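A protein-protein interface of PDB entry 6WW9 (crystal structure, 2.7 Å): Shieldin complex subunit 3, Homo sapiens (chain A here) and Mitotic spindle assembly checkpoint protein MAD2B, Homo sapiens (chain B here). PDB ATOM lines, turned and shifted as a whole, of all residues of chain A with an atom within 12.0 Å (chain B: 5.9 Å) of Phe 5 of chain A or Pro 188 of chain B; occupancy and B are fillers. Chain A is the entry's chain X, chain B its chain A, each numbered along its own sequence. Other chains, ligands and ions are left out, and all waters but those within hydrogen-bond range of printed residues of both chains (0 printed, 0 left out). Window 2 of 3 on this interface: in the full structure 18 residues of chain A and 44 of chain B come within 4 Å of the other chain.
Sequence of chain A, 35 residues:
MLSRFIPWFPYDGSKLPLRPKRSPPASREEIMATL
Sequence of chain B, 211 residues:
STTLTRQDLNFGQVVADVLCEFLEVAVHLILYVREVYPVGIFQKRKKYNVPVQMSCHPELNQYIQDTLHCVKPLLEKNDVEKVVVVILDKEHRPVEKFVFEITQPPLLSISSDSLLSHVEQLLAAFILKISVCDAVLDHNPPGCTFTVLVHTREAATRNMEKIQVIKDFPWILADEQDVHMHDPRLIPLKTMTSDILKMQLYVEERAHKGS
Among the printed residues, merely in contact across the chains: Phe 5 of chain A with Leu 186 of chain B, Phe 5 of chain A with Pro 188 of chain B, Phe 5 of chain A with Thr 191 of chain B, Phe 5 of chain A with Gln 200 of chain B, Phe 5 of chain A with Tyr 202 of chain B, Pro 7 of chain A with Glu 101 of chain B, Pro 7 of chain A with Gln 200 of chain B and Pro 7 of chain A with Tyr 202 of chain B.
Of chain B, only Leu 186 (3.9 Å), Pro 188 (3.5 Å), Thr 191 (3.1 Å), Gln 200 (3.2 Å) and Tyr 202 (3.6 Å) come within 4 Å of Phe 5 of chain A.
Of chain A, only Phe 5 (3.5 Å) comes within 4 Å of Pro 188 of chain B.
Of chain A, only Phe 5 (3.9 Å) comes within 4 Å of Leu 186 of chain B.
No residue of chain A comes within 4 Å of Ile 187 of chain B.
No residue of chain A comes within 4 Å of Leu 189 of chain B.
Of chain A, only Phe 5 (3.1 Å) comes within 4 Å of Thr 191 of chain B.
Printed residues of chain A within 4 Å of Gln 200 of chain B: Phe 5, Ile 6, Pro 7 and Trp 8.
Leu 201 of chain B touches none of the printed residues of chain A.
Tyr 202 of chain B touches just these residues of chain A: Phe 5 (3.6 Å) and Pro 7 (3.5 Å).
No residue of chain A comes within 4 Å of Val 203 of chain B.
Of the printed residues of chain B, Pro 7 of chain A touches Glu 101, Gln 200 and Tyr 202.
Of the printed residues of chain B, Phe 9 of chain A touches Glu 101 (3.0 Å).
Of the printed residues of chain B, Trp 8 of chain A touches Glu 101 and Gln 200.
Printed residues of chain A within 4 Å of Glu 101 of chain B: Pro 7, Trp 8 and Phe 9.
Of the printed residues of chain B, Ile 6 of chain A touches Gln 200.
Lys 190 of chain B touches none of the printed residues of chain A.
The nearest residue of chain B that does not touch Phe 5 of chain A is Lys 190 of chain B (4.8 Å).
Of the 7 printed residues of chain A, 5 touch a printed residue of chain B.
Hydrophobic or aromatic side chains of chain B within 4 Å of the printed part of chain A: Leu 186, Pro 188 and Tyr 202.
The side-chain amide nitrogen (NE2) of Gln 200 of chain B is in hydrogen-bond range of the side-chain carboxylate (OE1) of Glu 101 of chain B (2.6 Å).
The side-chain carboxylate (OE2) of Glu 101 of chain B lies within hydrogen-bond range of the side-chain hydroxyl (OH) of Tyr 202 of chain B (2.7 Å).
The side-chain amide oxygen (OE1) of Gln 200 of chain B is in hydrogen-bond range of the side-chain hydroxyl (OG1) of Thr 191 of chain B (2.9 Å).
The side-chain carboxylate (OE1) of Glu 101 of chain B lies within hydrogen-bond range of the backbone NH (N) of Trp 8 of chain A, at 2.7 Å.
OE2 of Glu 101 of chain B is in hydrogen-bond range of N of Phe 9 of chain A, 3.0 Å away.
NE2 of Gln 200 of chain B sits at hydrogen-bond distance from O of Ile 6 of chain A (3.2 Å).
The backbone NH (N) of Trp 8 of chain A sits close to the side-chain amide nitrogen (NE2) of Gln 200 of chain B (3.4 Å).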
ATOM      1  N   PHE A   5     -35.367   5.074  -8.401  1.00  0.00           N
ATOM      2  CA  PHE A   5     -34.353   4.137  -8.874  1.00  0.00           C
ATOM      3  C   PHE A   5     -34.025   3.088  -7.817  1.00  0.00           C
ATOM      4  O   PHE A   5     -33.690   3.420  -6.679  1.00  0.00           O
ATOM      5  CB  PHE A   5     -33.076   4.879  -9.279  1.00  0.00           C
ATOM      6  CG  PHE A   5     -31.953   3.969  -9.711  1.00  0.00           C
ATOM      7  CD1 PHE A   5     -31.012   3.517  -8.797  1.00  0.00           C
ATOM      8  CD2 PHE A   5     -31.840   3.569 -11.033  1.00  0.00           C
ATOM      9  CE1 PHE A   5     -29.982   2.683  -9.193  1.00  0.00           C
ATOM     10  CE2 PHE A   5     -30.810   2.734 -11.434  1.00  0.00           C
ATOM     11  CZ  PHE A   5     -29.882   2.291 -10.513  1.00  0.00           C
ATOM     12  N   ILE A   6     -34.113   1.821  -8.207  1.00  0.00           N
ATOM     13  CA  ILE A   6     -33.749   0.709  -7.333  1.00  0.00           C
ATOM     14  C   ILE A   6     -32.971  -0.315  -8.150  1.00  0.00           C
ATOM     15  O   ILE A   6     -33.349  -0.613  -9.293  1.00  0.00           O
ATOM     16  CB  ILE A   6     -34.988   0.075  -6.679  1.00  0.00           C
ATOM     17  CG1 ILE A   6     -36.072  -0.189  -7.726  1.00  0.00           C
ATOM     18  CG2 ILE A   6     -35.523   0.961  -5.558  1.00  0.00           C
ATOM     19  CD1 ILE A   6     -37.338  -0.787  -7.157  1.00  0.00           C
ATOM     20  N   PRO A   7     -31.879  -0.866  -7.620  1.00  0.00           N
ATOM     21  CA  PRO A   7     -31.146  -1.899  -8.360  1.00  0.00           C
ATOM     22  C   PRO A   7     -31.946  -3.190  -8.443  1.00  0.00           C
ATOM     23  O   PRO A   7     -32.608  -3.599  -7.486  1.00  0.00           O
ATOM     24  CB  PRO A   7     -29.867  -2.084  -7.537  1.00  0.00           C
ATOM     25  CG  PRO A   7     -30.256  -1.670  -6.158  1.00  0.00           C
ATOM     26  CD  PRO A   7     -31.238  -0.544  -6.335  1.00  0.00           C
ATOM     27  N   TRP A   8     -31.869  -3.837  -9.607  1.00  0.00           N
ATOM     28  CA  TRP A   8     -32.677  -5.023  -9.866  1.00  0.00           C
ATOM     29  C   TRP A   8     -32.141  -6.252  -9.142  1.00  0.00           C
ATOM     30  O   TRP A   8     -32.923  -7.077  -8.655  1.00  0.00           O
ATOM     31  CB  TRP A   8     -32.748  -5.282 -11.370  1.00  0.00           C
ATOM     32  CG  TRP A   8     -33.461  -4.205 -12.121  1.00  0.00           C
ATOM     33  CD1 TRP A   8     -34.303  -3.266 -11.601  1.00  0.00           C
ATOM     34  CD2 TRP A   8     -33.390  -3.948 -13.527  1.00  0.00           C
ATOM     35  NE1 TRP A   8     -34.766  -2.443 -12.598  1.00  0.00           N
ATOM     36  CE2 TRP A   8     -34.220  -2.840 -13.790  1.00  0.00           C
ATOM     37  CE3 TRP A   8     -32.708  -4.547 -14.590  1.00  0.00           C
ATOM     38  CZ2 TRP A   8     -34.387  -2.319 -15.072  1.00  0.00           C
ATOM     39  CZ3 TRP A   8     -32.875  -4.028 -15.862  1.00  0.00           C
ATOM     40  CH2 TRP A   8     -33.707  -2.925 -16.092  1.00  0.00           C
ATOM     41  N   PHE A   9     -30.818  -6.400  -9.068  1.00  0.00           N
ATOM     42  CA  PHE A   9     -30.181  -7.551  -8.429  1.00  0.00           C
ATOM     43  C   PHE A   9     -29.284  -7.046  -7.307  1.00  0.00           C
ATOM     44  O   PHE A   9     -28.088  -6.791  -7.523  1.00  0.00           O
ATOM     45  CB  PHE A   9     -29.390  -8.375  -9.440  1.00  0.00           C
ATOM     46  CG  PHE A   9     -30.113  -8.602 -10.735  1.00  0.00           C
ATOM     47  CD1 PHE A   9     -31.178  -9.485 -10.804  1.00  0.00           C
ATOM     48  CD2 PHE A   9     -29.724  -7.939 -11.887  1.00  0.00           C
ATOM     49  CE1 PHE A   9     -31.844  -9.697 -11.995  1.00  0.00           C
ATOM     50  CE2 PHE A   9     -30.385  -8.147 -13.082  1.00  0.00           C
ATOM     51  CZ  PHE A   9     -31.447  -9.026 -13.136  1.00  0.00           C
ATOM     52  N   PRO A  10     -29.819  -6.882  -6.098  1.00  0.00           N
ATOM     53  CA  PRO A  10     -28.993  -6.432  -4.973  1.00  0.00           C
ATOM     54  C   PRO A  10     -27.873  -7.419  -4.674  1.00  0.00           C
ATOM     55  O   PRO A  10     -27.926  -8.595  -5.039  1.00  0.00           O
ATOM     56  CB  PRO A  10     -29.991  -6.351  -3.811  1.00  0.00           C
ATOM     57  CG  PRO A  10     -31.328  -6.203  -4.469  1.00  0.00           C
ATOM     58  CD  PRO A  10     -31.240  -7.006  -5.732  1.00  0.00           C
ATOM     59  N   TYR A  11     -26.844  -6.917  -3.993  1.00  0.00           N
ATOM     60  CA  TYR A  11     -25.662  -7.725  -3.714  1.00  0.00           C
ATOM     61  C   TYR A  11     -26.019  -8.920  -2.838  1.00  0.00           C
ATOM     62  O   TYR A  11     -26.478  -8.753  -1.703  1.00  0.00           O
ATOM     63  CB  TYR A  11     -24.587  -6.869  -3.045  1.00  0.00           C
ATOM     64  CG  TYR A  11     -23.390  -7.668  -2.587  1.00  0.00           C
ATOM     65  CD1 TYR A  11     -22.665  -8.440  -3.485  1.00  0.00           C
ATOM     66  CD2 TYR A  11     -22.985  -7.653  -1.257  1.00  0.00           C
ATOM     67  CE1 TYR A  11     -21.573  -9.177  -3.073  1.00  0.00           C
ATOM     68  CE2 TYR A  11     -21.890  -8.387  -0.836  1.00  0.00           C
ATOM     69  CZ  TYR A  11     -21.189  -9.146  -1.750  1.00  0.00           C
ATOM     70  OH  TYR A  11     -20.100  -9.878  -1.344  1.00  0.00           O
ATOM     71  N   GLU B 101     -26.559  -4.147 -14.832  1.00  0.00           N
ATOM     72  CA  GLU B 101     -27.619  -5.119 -14.612  1.00  0.00           C
ATOM     73  C   GLU B 101     -28.334  -5.383 -15.932  1.00  0.00           C
ATOM     74  O   GLU B 101     -28.749  -4.447 -16.620  1.00  0.00           O
ATOM     75  CB  GLU B 101     -28.595  -4.613 -13.552  1.00  0.00           C
ATOM     76  CG  GLU B 101     -27.959  -4.405 -12.184  1.00  0.00           C
ATOM     77  CD  GLU B 101     -28.968  -4.015 -11.123  1.00  0.00           C
ATOM     78  OE1 GLU B 101     -29.969  -3.353 -11.467  1.00  0.00           O
ATOM     79  OE2 GLU B 101     -28.762  -4.375  -9.944  1.00  0.00           O
ATOM     80  N   LEU B 186     -24.223   4.972  -3.870  1.00  0.00           N
ATOM     81  CA  LEU B 186     -24.826   4.486  -5.107  1.00  0.00           C
ATOM     82  C   LEU B 186     -25.054   5.661  -6.048  1.00  0.00           C
ATOM     83  O   LEU B 186     -25.782   6.601  -5.709  1.00  0.00           O
ATOM     84  CB  LEU B 186     -26.142   3.758  -4.835  1.00  0.00           C
ATOM     85  CG  LEU B 186     -26.500   2.685  -5.869  1.00  0.00           C
ATOM     86  CD1 LEU B 186     -25.679   1.421  -5.627  1.00  0.00           C
ATOM     87  CD2 LEU B 186     -27.996   2.380  -5.889  1.00  0.00           C
ATOM     88  N   ILE B 187     -24.437   5.603  -7.226  1.00  0.00           N
ATOM     89  CA  ILE B 187     -24.583   6.649  -8.235  1.00  0.00           C
ATOM     90  C   ILE B 187     -25.339   6.088  -9.433  1.00  0.00           C
ATOM     91  O   ILE B 187     -24.729   5.451 -10.306  1.00  0.00           O
ATOM     92  CB  ILE B 187     -23.219   7.207  -8.669  1.00  0.00           C
ATOM     93  CG1 ILE B 187     -22.355   7.522  -7.448  1.00  0.00           C
ATOM     94  CG2 ILE B 187     -23.407   8.453  -9.520  1.00  0.00           C
ATOM     95  CD1 ILE B 187     -22.969   8.541  -6.519  1.00  0.00           C
ATOM     96  N   PRO B 188     -26.652   6.286  -9.517  1.00  0.00           N
ATOM     97  CA  PRO B 188     -27.385   5.830 -10.703  1.00  0.00           C
ATOM     98  C   PRO B 188     -26.962   6.615 -11.933  1.00  0.00           C
ATOM     99  O   PRO B 188     -26.828   7.840 -11.895  1.00  0.00           O
ATOM    100  CB  PRO B 188     -28.853   6.097 -10.346  1.00  0.00           C
ATOM    101  CG  PRO B 188     -28.872   6.261  -8.862  1.00  0.00           C
ATOM    102  CD  PRO B 188     -27.549   6.847  -8.495  1.00  0.00           C
ATOM    103  N   LEU B 189     -26.745   5.893 -13.032  1.00  0.00           N
ATOM    104  CA  LEU B 189     -26.389   6.510 -14.303  1.00  0.00           C
ATOM    105  C   LEU B 189     -27.535   6.451 -15.306  1.00  0.00           C
ATOM    106  O   LEU B 189     -27.979   7.497 -15.787  1.00  0.00           O
ATOM    107  CB  LEU B 189     -25.126   5.854 -14.884  1.00  0.00           C
ATOM    108  CG  LEU B 189     -23.827   6.137 -14.122  1.00  0.00           C
ATOM    109  CD1 LEU B 189     -22.617   5.557 -14.843  1.00  0.00           C
ATOM    110  CD2 LEU B 189     -23.649   7.633 -13.895  1.00  0.00           C
ATOM    111  N   LYS B 190     -28.039   5.262 -15.633  1.00  0.00           N
ATOM    112  CA  LYS B 190     -29.123   5.161 -16.599  1.00  0.00           C
ATOM    113  C   LYS B 190     -29.913   3.876 -16.389  1.00  0.00           C
ATOM    114  O   LYS B 190     -29.346   2.832 -16.056  1.00  0.00           O
ATOM    115  CB  LYS B 190     -28.605   5.215 -18.040  1.00  0.00           C
ATOM    116  CG  LYS B 190     -29.667   5.673 -19.018  1.00  0.00           C
ATOM    117  CD  LYS B 190     -29.261   5.475 -20.460  1.00  0.00           C
ATOM    118  CE  LYS B 190     -30.379   5.941 -21.374  1.00  0.00           C
ATOM    119  NZ  LYS B 190     -30.631   7.401 -21.219  1.00  0.00           N
ATOM    120  N   THR B 191     -31.226   3.970 -16.589  1.00  0.00           N
ATOM    121  CA  THR B 191     -32.127   2.825 -16.559  1.00  0.00           C
ATOM    122  C   THR B 191     -32.937   2.826 -17.844  1.00  0.00           C
ATOM    123  O   THR B 191     -33.482   3.864 -18.235  1.00  0.00           O
ATOM    124  CB  THR B 191     -33.062   2.873 -15.338  1.00  0.00           C
ATOM    125  OG1 THR B 191     -32.290   2.790 -14.133  1.00  0.00           O
ATOM    126  CG2 THR B 191     -34.050   1.718 -15.373  1.00  0.00           C
ATOM    127  N   GLN B 200     -29.749  -1.651 -16.526  1.00  0.00           N
ATOM    128  CA  GLN B 200     -29.418  -0.557 -15.628  1.00  0.00           C
ATOM    129  C   GLN B 200     -27.906  -0.430 -15.509  1.00  0.00           C
ATOM    130  O   GLN B 200     -27.184  -1.433 -15.526  1.00  0.00           O
ATOM    131  CB  GLN B 200     -30.022  -0.765 -14.240  1.00  0.00           C
ATOM    132  CG  GLN B 200     -31.517  -0.559 -14.175  1.00  0.00           C
ATOM    133  CD  GLN B 200     -32.019  -0.452 -12.750  1.00  0.00           C
ATOM    134  OE1 GLN B 200     -32.791   0.448 -12.417  1.00  0.00           O
ATOM    135  NE2 GLN B 200     -31.580  -1.371 -11.896  1.00  0.00           N
ATOM    136  N   LEU B 201     -27.439   0.808 -15.382  1.00  0.00           N
ATOM    137  CA  LEU B 201     -26.033   1.100 -15.146  1.00  0.00           C
ATOM    138  C   LEU B 201     -25.941   2.061 -13.975  1.00  0.00           C
ATOM    139  O   LEU B 201     -26.522   3.150 -14.018  1.00  0.00           O
ATOM    140  CB  LEU B 201     -25.370   1.698 -16.389  1.00  0.00           C
ATOM    141  CG  LEU B 201     -23.978   2.292 -16.172  1.00  0.00           C
ATOM    142  CD1 LEU B 201     -23.006   1.233 -15.681  1.00  0.00           C
ATOM    143  CD2 LEU B 201     -23.471   2.935 -17.448  1.00  0.00           C
ATOM    144  N   TYR B 202     -25.227   1.658 -12.927  1.00  0.00           N
ATOM    145  CA  TYR B 202     -25.001   2.532 -11.789  1.00  0.00           C
ATOM    146  C   TYR B 202     -23.611   2.259 -11.234  1.00  0.00           C
ATOM    147  O   TYR B 202     -22.932   1.310 -11.634  1.00  0.00           O
ATOM    148  CB  TYR B 202     -26.080   2.355 -10.714  1.00  0.00           C
ATOM    149  CG  TYR B 202     -26.244   0.939 -10.215  1.00  0.00           C
ATOM    150  CD1 TYR B 202     -27.103   0.053 -10.851  1.00  0.00           C
ATOM    151  CD2 TYR B 202     -25.545   0.490  -9.102  1.00  0.00           C
ATOM    152  CE1 TYR B 202     -27.257  -1.240 -10.396  1.00  0.00           C
ATOM    153  CE2 TYR B 202     -25.691  -0.801  -8.641  1.00  0.00           C
ATOM    154  CZ  TYR B 202     -26.549  -1.661  -9.291  1.00  0.00           C
ATOM    155  OH  TYR B 202     -26.699  -2.949  -8.834  1.00  0.00           O
ATOM    156  N   VAL B 203     -23.189   3.114 -10.306  1.00  0.00           N
ATOM    157  CA  VAL B 203     -21.846   3.067  -9.746  1.00  0.00           C
ATOM    158  C   VAL B 203     -21.942   2.893  -8.238  1.00  0.00           C
ATOM    159  O   VAL B 203     -22.674   3.631  -7.569  1.00  0.00           O
ATOM    160  CB  VAL B 203     -21.044   4.334 -10.094  1.00  0.00           C
ATOM    161  CG1 VAL B 203     -19.602   4.191  -9.624  1.00  0.00           C
ATOM    162  CG2 VAL B 203     -21.110   4.599 -11.585  1.00  0.00           C
